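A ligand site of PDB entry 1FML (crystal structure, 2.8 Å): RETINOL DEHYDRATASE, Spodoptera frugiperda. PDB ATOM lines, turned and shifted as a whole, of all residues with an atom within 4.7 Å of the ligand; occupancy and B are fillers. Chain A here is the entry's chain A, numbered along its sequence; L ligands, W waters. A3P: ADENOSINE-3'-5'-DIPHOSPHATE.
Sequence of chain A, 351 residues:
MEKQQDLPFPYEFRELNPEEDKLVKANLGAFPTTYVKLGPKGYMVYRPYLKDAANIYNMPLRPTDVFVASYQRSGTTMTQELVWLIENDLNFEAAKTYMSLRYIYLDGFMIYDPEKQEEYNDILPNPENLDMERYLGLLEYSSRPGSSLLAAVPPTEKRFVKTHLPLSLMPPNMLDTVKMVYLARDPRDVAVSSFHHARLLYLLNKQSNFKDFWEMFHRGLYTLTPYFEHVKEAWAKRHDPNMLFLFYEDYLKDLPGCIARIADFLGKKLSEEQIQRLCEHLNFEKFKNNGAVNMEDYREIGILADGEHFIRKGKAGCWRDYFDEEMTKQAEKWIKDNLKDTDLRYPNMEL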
ATOM      1  N   SER A  70      -7.999 -25.678 -16.791  1.00  0.00           N
ATOM      2  CA  SER A  70      -8.822 -26.055 -17.936  1.00  0.00           C
ATOM      3  C   SER A  70      -7.948 -26.528 -19.069  1.00  0.00           C
ATOM      4  O   SER A  70      -6.761 -26.212 -19.123  1.00  0.00           O
ATOM      5  CB  SER A  70      -9.576 -24.846 -18.468  1.00  0.00           C
ATOM      6  OG  SER A  70      -8.678 -24.029 -19.209  1.00  0.00           O
ATOM      7  N   GLN A  72      -6.886 -25.925 -22.582  1.00  0.00           N
ATOM      8  CA  GLN A  72      -6.900 -24.646 -23.282  1.00  0.00           C
ATOM      9  C   GLN A  72      -8.079 -24.362 -24.211  1.00  0.00           C
ATOM     10  O   GLN A  72      -8.614 -25.269 -24.838  1.00  0.00           O
ATOM     11  CB  GLN A  72      -5.615 -24.501 -24.087  1.00  0.00           C
ATOM     12  CG  GLN A  72      -5.382 -25.688 -24.969  1.00  0.00           C
ATOM     13  CD  GLN A  72      -4.384 -25.393 -26.037  1.00  0.00           C
ATOM     14  OE1 GLN A  72      -4.747 -25.036 -27.156  1.00  0.00           O
ATOM     15  NE2 GLN A  72      -3.100 -25.507 -25.700  1.00  0.00           N
ATOM     16  N   ARG A  73      -8.456 -23.094 -24.313  1.00  0.00           N
ATOM     17  CA  ARG A  73      -9.544 -22.623 -25.171  1.00  0.00           C
ATOM     18  C   ARG A  73     -10.946 -23.013 -24.719  1.00  0.00           C
ATOM     19  O   ARG A  73     -11.842 -23.150 -25.553  1.00  0.00           O
ATOM     20  CB  ARG A  73      -9.330 -23.093 -26.622  1.00  0.00           C
ATOM     21  CG  ARG A  73      -7.919 -22.851 -27.139  1.00  0.00           C
ATOM     22  CD  ARG A  73      -7.501 -21.421 -26.906  1.00  0.00           C
ATOM     23  NE  ARG A  73      -8.217 -20.516 -27.783  1.00  0.00           N
ATOM     24  CZ  ARG A  73      -8.275 -19.200 -27.626  1.00  0.00           C
ATOM     25  NH1 ARG A  73      -7.660 -18.621 -26.596  1.00  0.00           N
ATOM     26  NH2 ARG A  73      -8.934 -18.453 -28.500  1.00  0.00           N
ATOM     27  N   SER A  74     -11.135 -23.171 -23.415  1.00  0.00           N
ATOM     28  CA  SER A  74     -12.431 -23.559 -22.869  1.00  0.00           C
ATOM     29  C   SER A  74     -13.063 -22.468 -22.010  1.00  0.00           C
ATOM     30  O   SER A  74     -14.138 -22.681 -21.427  1.00  0.00           O
ATOM     31  CB  SER A  74     -12.299 -24.831 -22.017  1.00  0.00           C
ATOM     32  OG  SER A  74     -11.712 -25.905 -22.750  1.00  0.00           O
ATOM     33  N   GLY A  75     -12.422 -21.295 -21.916  1.00  0.00           N
ATOM     34  CA  GLY A  75     -12.979 -20.229 -21.104  1.00  0.00           C
ATOM     35  C   GLY A  75     -12.079 -19.707 -20.005  1.00  0.00           C
ATOM     36  O   GLY A  75     -12.519 -18.952 -19.113  1.00  0.00           O
ATOM     37  N   THR A  76     -10.805 -20.097 -20.045  1.00  0.00           N
ATOM     38  CA  THR A  76      -9.852 -19.676 -19.030  1.00  0.00           C
ATOM     39  C   THR A  76      -9.881 -18.174 -18.818  1.00  0.00           C
ATOM     40  O   THR A  76     -10.123 -17.708 -17.709  1.00  0.00           O
ATOM     41  CB  THR A  76      -8.423 -20.060 -19.411  1.00  0.00           C
ATOM     42  OG1 THR A  76      -8.431 -21.290 -20.142  1.00  0.00           O
ATOM     43  CG2 THR A  76      -7.573 -20.228 -18.161  1.00  0.00           C
ATOM     44  N   THR A  77      -9.634 -17.404 -19.883  1.00  0.00           N
ATOM     45  CA  THR A  77      -9.593 -15.942 -19.804  1.00  0.00           C
ATOM     46  C   THR A  77     -10.801 -15.340 -19.122  1.00  0.00           C
ATOM     47  O   THR A  77     -10.651 -14.606 -18.138  1.00  0.00           O
ATOM     48  CB  THR A  77      -9.415 -15.322 -21.202  1.00  0.00           C
ATOM     49  OG1 THR A  77      -8.424 -16.048 -21.932  1.00  0.00           O
ATOM     50  CG2 THR A  77      -8.933 -13.891 -21.083  1.00  0.00           C
ATOM     51  N   MET A  78     -12.006 -15.637 -19.620  1.00  0.00           N
ATOM     52  CA  MET A  78     -13.236 -15.130 -18.999  1.00  0.00           C
ATOM     53  C   MET A  78     -13.183 -15.378 -17.498  1.00  0.00           C
ATOM     54  O   MET A  78     -13.365 -14.485 -16.688  1.00  0.00           O
ATOM     55  CB  MET A  78     -14.465 -15.877 -19.511  1.00  0.00           C
ATOM     56  CG  MET A  78     -14.650 -15.848 -20.991  1.00  0.00           C
ATOM     57  SD  MET A  78     -16.144 -16.722 -21.426  1.00  0.00           S
ATOM     58  CE  MET A  78     -17.372 -15.668 -20.699  1.00  0.00           C
ATOM     59  N   ARG A 185     -15.230 -27.467 -22.232  1.00  0.00           N
ATOM     60  CA  ARG A 185     -15.994 -27.003 -23.378  1.00  0.00           C
ATOM     61  C   ARG A 185     -16.084 -28.135 -24.380  1.00  0.00           C
ATOM     62  O   ARG A 185     -15.249 -29.035 -24.372  1.00  0.00           O
ATOM     63  CB  ARG A 185     -15.277 -25.809 -24.014  1.00  0.00           C
ATOM     64  CG  ARG A 185     -15.940 -25.211 -25.226  1.00  0.00           C
ATOM     65  CD  ARG A 185     -14.975 -24.270 -25.947  1.00  0.00           C
ATOM     66  NE  ARG A 185     -15.666 -23.357 -26.843  1.00  0.00           N
ATOM     67  CZ  ARG A 185     -15.083 -22.368 -27.507  1.00  0.00           C
ATOM     68  NH1 ARG A 185     -13.784 -22.157 -27.389  1.00  0.00           N
ATOM     69  NH2 ARG A 185     -15.808 -21.571 -28.269  1.00  0.00           N
ATOM     70  N   SER A 193     -11.121 -23.733 -31.998  1.00  0.00           N
ATOM     71  CA  SER A 193     -10.454 -22.599 -31.370  1.00  0.00           C
ATOM     72  C   SER A 193      -8.967 -22.800 -31.269  1.00  0.00           C
ATOM     73  O   SER A 193      -8.208 -21.854 -31.443  1.00  0.00           O
ATOM     74  CB  SER A 193     -11.009 -22.348 -29.987  1.00  0.00           C
ATOM     75  OG  SER A 193     -10.459 -21.154 -29.460  1.00  0.00           O
ATOM     76  N   TYR A 248     -18.152 -23.978 -20.592  1.00  0.00           N
ATOM     77  CA  TYR A 248     -18.089 -22.762 -21.386  1.00  0.00           C
ATOM     78  C   TYR A 248     -19.446 -22.439 -22.001  1.00  0.00           C
ATOM     79  O   TYR A 248     -19.805 -21.279 -22.174  1.00  0.00           O
ATOM     80  CB  TYR A 248     -17.084 -22.928 -22.518  1.00  0.00           C
ATOM     81  CG  TYR A 248     -17.056 -21.747 -23.467  1.00  0.00           C
ATOM     82  CD1 TYR A 248     -16.416 -20.560 -23.132  1.00  0.00           C
ATOM     83  CD2 TYR A 248     -17.714 -21.814 -24.696  1.00  0.00           C
ATOM     84  CE1 TYR A 248     -16.441 -19.451 -23.984  1.00  0.00           C
ATOM     85  CE2 TYR A 248     -17.752 -20.722 -25.568  1.00  0.00           C
ATOM     86  CZ  TYR A 248     -17.121 -19.546 -25.204  1.00  0.00           C
ATOM     87  OH  TYR A 248     -17.181 -18.473 -26.066  1.00  0.00           O
ATOM     88  N   LEU A 252     -22.384 -18.871 -21.812  1.00  0.00           N
ATOM     89  CA  LEU A 252     -23.158 -18.250 -22.870  1.00  0.00           C
ATOM     90  C   LEU A 252     -24.648 -18.357 -22.586  1.00  0.00           C
ATOM     91  O   LEU A 252     -25.399 -17.436 -22.899  1.00  0.00           O
ATOM     92  CB  LEU A 252     -22.854 -18.919 -24.213  1.00  0.00           C
ATOM     93  CG  LEU A 252     -21.397 -18.965 -24.721  1.00  0.00           C
ATOM     94  CD1 LEU A 252     -21.370 -19.570 -26.105  1.00  0.00           C
ATOM     95  CD2 LEU A 252     -20.803 -17.577 -24.743  1.00  0.00           C
ATOM     96  N   LEU A 282     -18.204  -8.474 -19.097  1.00  0.00           N
ATOM     97  CA  LEU A 282     -17.793  -9.671 -19.813  1.00  0.00           C
ATOM     98  C   LEU A 282     -18.433  -9.770 -21.186  1.00  0.00           C
ATOM     99  O   LEU A 282     -18.380 -10.833 -21.805  1.00  0.00           O
ATOM    100  CB  LEU A 282     -18.144 -10.928 -18.995  1.00  0.00           C
ATOM    101  CG  LEU A 282     -17.032 -11.561 -18.157  1.00  0.00           C
ATOM    102  CD1 LEU A 282     -16.088 -12.320 -19.062  1.00  0.00           C
ATOM    103  CD2 LEU A 282     -16.296 -10.506 -17.361  1.00  0.00           C
ATOM    104  N   ASN A 283     -19.047  -8.683 -21.648  1.00  0.00           N
ATOM    105  CA  ASN A 283     -19.673  -8.686 -22.965  1.00  0.00           C
ATOM    106  C   ASN A 283     -18.577  -9.074 -23.939  1.00  0.00           C
ATOM    107  O   ASN A 283     -17.453  -8.581 -23.820  1.00  0.00           O
ATOM    108  CB  ASN A 283     -20.216  -7.293 -23.298  1.00  0.00           C
ATOM    109  CG  ASN A 283     -20.785  -7.196 -24.696  1.00  0.00           C
ATOM    110  OD1 ASN A 283     -20.046  -7.211 -25.682  1.00  0.00           O
ATOM    111  ND2 ASN A 283     -22.108  -7.094 -24.795  1.00  0.00           N
ATOM    112  N   PHE A 284     -18.879  -9.955 -24.891  1.00  0.00           N
ATOM    113  CA  PHE A 284     -17.852 -10.388 -25.827  1.00  0.00           C
ATOM    114  C   PHE A 284     -17.088  -9.267 -26.514  1.00  0.00           C
ATOM    115  O   PHE A 284     -15.857  -9.216 -26.441  1.00  0.00           O
ATOM    116  CB  PHE A 284     -18.429 -11.301 -26.901  1.00  0.00           C
ATOM    117  CG  PHE A 284     -17.385 -12.018 -27.692  1.00  0.00           C
ATOM    118  CD1 PHE A 284     -16.570 -12.976 -27.085  1.00  0.00           C
ATOM    119  CD2 PHE A 284     -17.140 -11.683 -29.020  1.00  0.00           C
ATOM    120  CE1 PHE A 284     -15.532 -13.578 -27.784  1.00  0.00           C
ATOM    121  CE2 PHE A 284     -16.105 -12.284 -29.734  1.00  0.00           C
ATOM    122  CZ  PHE A 284     -15.299 -13.232 -29.109  1.00  0.00           C
ATOM    123  N   PHE A 287     -15.025  -7.243 -24.172  1.00  0.00           N
ATOM    124  CA  PHE A 287     -13.871  -8.035 -23.725  1.00  0.00           C
ATOM    125  C   PHE A 287     -12.843  -8.123 -24.854  1.00  0.00           C
ATOM    126  O   PHE A 287     -11.679  -7.800 -24.671  1.00  0.00           O
ATOM    127  CB  PHE A 287     -14.343  -9.422 -23.322  1.00  0.00           C
ATOM    128  CG  PHE A 287     -13.551 -10.038 -22.216  1.00  0.00           C
ATOM    129  CD1 PHE A 287     -13.496  -9.422 -20.971  1.00  0.00           C
ATOM    130  CD2 PHE A 287     -12.836 -11.212 -22.418  1.00  0.00           C
ATOM    131  CE1 PHE A 287     -12.749  -9.978 -19.931  1.00  0.00           C
ATOM    132  CE2 PHE A 287     -12.083 -11.769 -21.386  1.00  0.00           C
ATOM    133  CZ  PHE A 287     -12.034 -11.153 -20.133  1.00  0.00           C
ATOM    134  N   PHE A 310      -6.597 -13.479 -29.978  1.00  0.00           N
ATOM    135  CA  PHE A 310      -6.735 -14.329 -28.804  1.00  0.00           C
ATOM    136  C   PHE A 310      -8.200 -14.476 -28.420  1.00  0.00           C
ATOM    137  O   PHE A 310      -8.592 -15.453 -27.786  1.00  0.00           O
ATOM    138  CB  PHE A 310      -5.942 -13.740 -27.620  1.00  0.00           C
ATOM    139  CG  PHE A 310      -5.880 -14.654 -26.433  1.00  0.00           C
ATOM    140  CD1 PHE A 310      -5.291 -15.912 -26.539  1.00  0.00           C
ATOM    141  CD2 PHE A 310      -6.426 -14.273 -25.214  1.00  0.00           C
ATOM    142  CE1 PHE A 310      -5.257 -16.776 -25.443  1.00  0.00           C
ATOM    143  CE2 PHE A 310      -6.397 -15.127 -24.109  1.00  0.00           C
ATOM    144  CZ  PHE A 310      -5.811 -16.383 -24.228  1.00  0.00           C
ATOM    145  N   ILE A 311      -9.008 -13.503 -28.818  1.00  0.00           N
ATOM    146  CA  ILE A 311     -10.448 -13.523 -28.550  1.00  0.00           C
ATOM    147  C   ILE A 311     -11.140 -13.435 -29.911  1.00  0.00           C
ATOM    148  O   ILE A 311     -11.183 -12.372 -30.509  1.00  0.00           O
ATOM    149  CB  ILE A 311     -10.832 -12.331 -27.659  1.00  0.00           C
ATOM    150  CG1 ILE A 311     -10.044 -12.435 -26.355  1.00  0.00           C
ATOM    151  CG2 ILE A 311     -12.312 -12.337 -27.382  1.00  0.00           C
ATOM    152  CD1 ILE A 311     -10.348 -11.392 -25.327  1.00  0.00           C
ATOM    153  N   ARG A 312     -11.673 -14.554 -30.390  1.00  0.00           N
ATOM    154  CA  ARG A 312     -12.318 -14.596 -31.706  1.00  0.00           C
ATOM    155  C   ARG A 312     -13.809 -14.344 -31.810  1.00  0.00           C
ATOM    156  O   ARG A 312     -14.259 -13.210 -31.887  1.00  0.00           O
ATOM    157  CB  ARG A 312     -12.058 -15.951 -32.378  1.00  0.00           C
ATOM    158  CG  ARG A 312     -10.674 -16.209 -32.898  1.00  0.00           C
ATOM    159  CD  ARG A 312     -10.747 -17.443 -33.768  1.00  0.00           C
ATOM    160  NE  ARG A 312     -11.543 -18.488 -33.125  1.00  0.00           N
ATOM    161  CZ  ARG A 312     -12.553 -19.144 -33.708  1.00  0.00           C
ATOM    162  NH1 ARG A 312     -12.886 -18.871 -34.964  1.00  0.00           N
ATOM    163  NH2 ARG A 312     -13.207 -20.075 -33.033  1.00  0.00           N
ATOM    164  N   LYS A 313     -14.574 -15.437 -31.843  1.00  0.00           N
ATOM    165  CA  LYS A 313     -16.016 -15.379 -31.973  1.00  0.00           C
ATOM    166  C   LYS A 313     -16.783 -15.485 -30.645  1.00  0.00           C
ATOM    167  O   LYS A 313     -17.718 -14.712 -30.406  1.00  0.00           O
ATOM    168  CB  LYS A 313     -16.478 -16.485 -32.922  1.00  0.00           C
ATOM    169  CG  LYS A 313     -15.998 -16.290 -34.344  1.00  0.00           C
ATOM    170  CD  LYS A 313     -16.430 -14.927 -34.868  1.00  0.00           C
ATOM    171  CE  LYS A 313     -16.321 -14.826 -36.393  1.00  0.00           C
ATOM    172  NZ  LYS A 313     -14.935 -14.984 -36.912  1.00  0.00           N
ATOM    173  N   GLY A 314     -16.377 -16.425 -29.782  1.00  0.00           N
ATOM    174  CA  GLY A 314     -17.057 -16.578 -28.504  1.00  0.00           C
ATOM    175  C   GLY A 314     -18.452 -17.125 -28.719  1.00  0.00           C
ATOM    176  O   GLY A 314     -19.390 -16.756 -28.023  1.00  0.00           O
ATOM    177  N   LYS A 315     -18.568 -18.003 -29.715  1.00  0.00           N
ATOM    178  CA  LYS A 315     -19.821 -18.626 -30.088  1.00  0.00           C
ATOM    179  C   LYS A 315     -19.804 -20.088 -29.672  1.00  0.00           C
ATOM    180  O   LYS A 315     -18.754 -20.631 -29.319  1.00  0.00           O
ATOM    181  CB  LYS A 315     -20.031 -18.530 -31.608  1.00  0.00           C
ATOM    182  CG  LYS A 315     -19.878 -17.116 -32.199  1.00  0.00           C
ATOM    183  CD  LYS A 315     -21.205 -16.341 -32.244  1.00  0.00           C
ATOM    184  CE  LYS A 315     -20.991 -14.868 -32.604  1.00  0.00           C
ATOM    185  NZ  LYS A 315     -20.197 -14.640 -33.854  1.00  0.00           N
HETATM  186  P1  A3P L   1     -13.442 -19.175 -29.701  1.00  0.00           P
HETATM  187  O1P A3P L   1     -12.162 -19.552 -30.385  1.00  0.00           O
HETATM  188  O2P A3P L   1     -13.853 -17.795 -30.054  1.00  0.00           O
HETATM  189  O3P A3P L   1     -14.512 -20.182 -30.058  1.00  0.00           O
HETATM  190  P2  A3P L   1      -9.436 -19.724 -23.327  1.00  0.00           P
HETATM  191  O4P A3P L   1      -9.428 -18.369 -22.658  1.00  0.00           O
HETATM  192  O5P A3P L   1      -9.615 -20.840 -22.335  1.00  0.00           O
HETATM  193  O6P A3P L   1      -8.170 -19.921 -24.130  1.00  0.00           O
HETATM  194  O5' A3P L   1     -10.672 -19.782 -24.340  1.00  0.00           O
HETATM  195  C5' A3P L   1     -10.790 -18.880 -25.408  1.00  0.00           C
HETATM  196  C4' A3P L   1     -12.195 -18.968 -25.993  1.00  0.00           C
HETATM  197  O4' A3P L   1     -13.086 -18.148 -25.173  1.00  0.00           O
HETATM  198  C3' A3P L   1     -12.305 -18.407 -27.390  1.00  0.00           C
HETATM  199  O3' A3P L   1     -13.250 -19.223 -28.108  1.00  0.00           O
HETATM  200  C2' A3P L   1     -12.711 -16.959 -27.116  1.00  0.00           C
HETATM  201  O2' A3P L   1     -13.195 -16.187 -28.210  1.00  0.00           O
HETATM  202  C1' A3P L   1     -13.707 -17.158 -25.975  1.00  0.00           C
HETATM  203  N9  A3P L   1     -13.915 -15.971 -25.148  1.00  0.00           N
HETATM  204  C8  A3P L   1     -12.980 -15.082 -24.616  1.00  0.00           C
HETATM  205  N7  A3P L   1     -13.485 -14.096 -23.901  1.00  0.00           N
HETATM  206  C5  A3P L   1     -14.861 -14.354 -23.949  1.00  0.00           C
HETATM  207  C6  A3P L   1     -16.001 -13.681 -23.389  1.00  0.00           C
HETATM  208  N6  A3P L   1     -15.883 -12.576 -22.634  1.00  0.00           N
HETATM  209  N1  A3P L   1     -17.305 -14.217 -23.628  1.00  0.00           N
HETATM  210  C2  A3P L   1     -17.450 -15.349 -24.402  1.00  0.00           C
HETATM  211  N3  A3P L   1     -16.418 -16.078 -24.997  1.00  0.00           N
HETATM  212  C4  A3P L   1     -15.155 -15.520 -24.726  1.00  0.00           C
HETATM  213  O   HOH W   1     -11.894 -17.351 -22.645  1.00  0.00           O
HETATM  214  O   HOH W   2      -5.883 -20.796 -23.566  1.00  0.00           O
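OG of Ser 193 sits at hydrogen-bond distance from O1P of the ligand (2.5 Å).
The backbone NH of Thr 76 sits at hydrogen-bond distance from an oxygen (O5P) of the ligand (2.7 Å).
OG1 of Thr 76 lies within hydrogen-bond range of O5P of the ligand, 2.5 Å away.
The guanidinium group (NH2) of Arg 185 lies within salt-bridge range of an oxygen (O3P) of the ligand.
The backbone NH (N) of Thr 77 is in hydrogen-bond range of an oxygen (O4P) of the ligand, at 2.9 Å.
The side-chain hydroxyl of Thr 77 lies within hydrogen-bond range of an oxygen (O4P) of the ligand (2.6 Å).
N3 of the ligand sits at hydrogen-bond distance from OH of Tyr 248 (2.7 Å).
An oxygen (O6P) of the ligand lies within hydrogen-bond range of the backbone NH (N) of Arg 73 (3.2 Å).
The guanidinium group of Arg 73 is in salt-bridge range of an oxygen (O6P) of the ligand (2.8 Å).
The backbone NH (N) of Gly 75 lies within hydrogen-bond range of an oxygen (O5P) of the ligand.
The backbone NH (N) of Gly 314 is in hydrogen-bond range of an oxygen (O2P) of the ligand (2.9 Å).
The backbone NH (N) of Arg 312 sits at hydrogen-bond distance from an oxygen (O2') of the ligand (3.1 Å).
NH2 of Arg 312 is in salt-bridge range of O1P of the ligand (2.9 Å).
The backbone NH (N) of Ser 74 sits at hydrogen-bond distance from an oxygen (O5P) of the ligand, 3.0 Å away.
The backbone NH (N) of Lys 313 sits at hydrogen-bond distance from an oxygen (O2P) of the ligand (3.0 Å).
The backbone carbonyl oxygen (O) of Leu 282 is in hydrogen-bond range of a nitrogen (N6) of the ligand (3.2 Å).
OG of Ser 193 sits at hydrogen-bond distance from NE of Arg 73, at 2.9 Å.
OG1 of Thr 76 sits at hydrogen-bond distance from OG of Ser 70, at 2.9 Å.
The backbone carbonyl oxygen (O) of Arg 73 sits at hydrogen-bond distance from the guanidinium group (NH1) of Arg 185, at 2.9 Å.
The guanidinium group of Arg 185 lies within hydrogen-bond range of the backbone carbonyl oxygen of Lys 315, at 3.3 Å.
The backbone carbonyl oxygen (O) of Gly 314 sits close to the side-chain hydroxyl (OH) of Tyr 248, 3.4 Å away.
The guanidinium group (NH2) of Arg 73 lies within hydrogen-bond range of the backbone carbonyl oxygen (O) of Phe 310.
SD of Met 78 lies close to N1 of the ligand, at 3.5 Å.
Residues that only touch the ligand: Phe 284 (3.5 Å), Phe 287 (3.3 Å) and Ile 311 (3.8 Å).
Hydrophobic or aromatic side chains within 4 Å of the ligand: Met 78, Tyr 248, Leu 282, Phe 284, Phe 287 and Ile 311.
Of the 22 residues printed, 16 come within 4 Å of the ligand.
Along chain A the residues within 4 Å of the ligand span positions 73 to 314.
The nearest printed residue that does not touch the ligand is Leu 252 (4.04 Å).
Water W1 lies within hydrogen-bond range of an oxygen (O4P) of the ligand and the backbone NH of Met 78.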
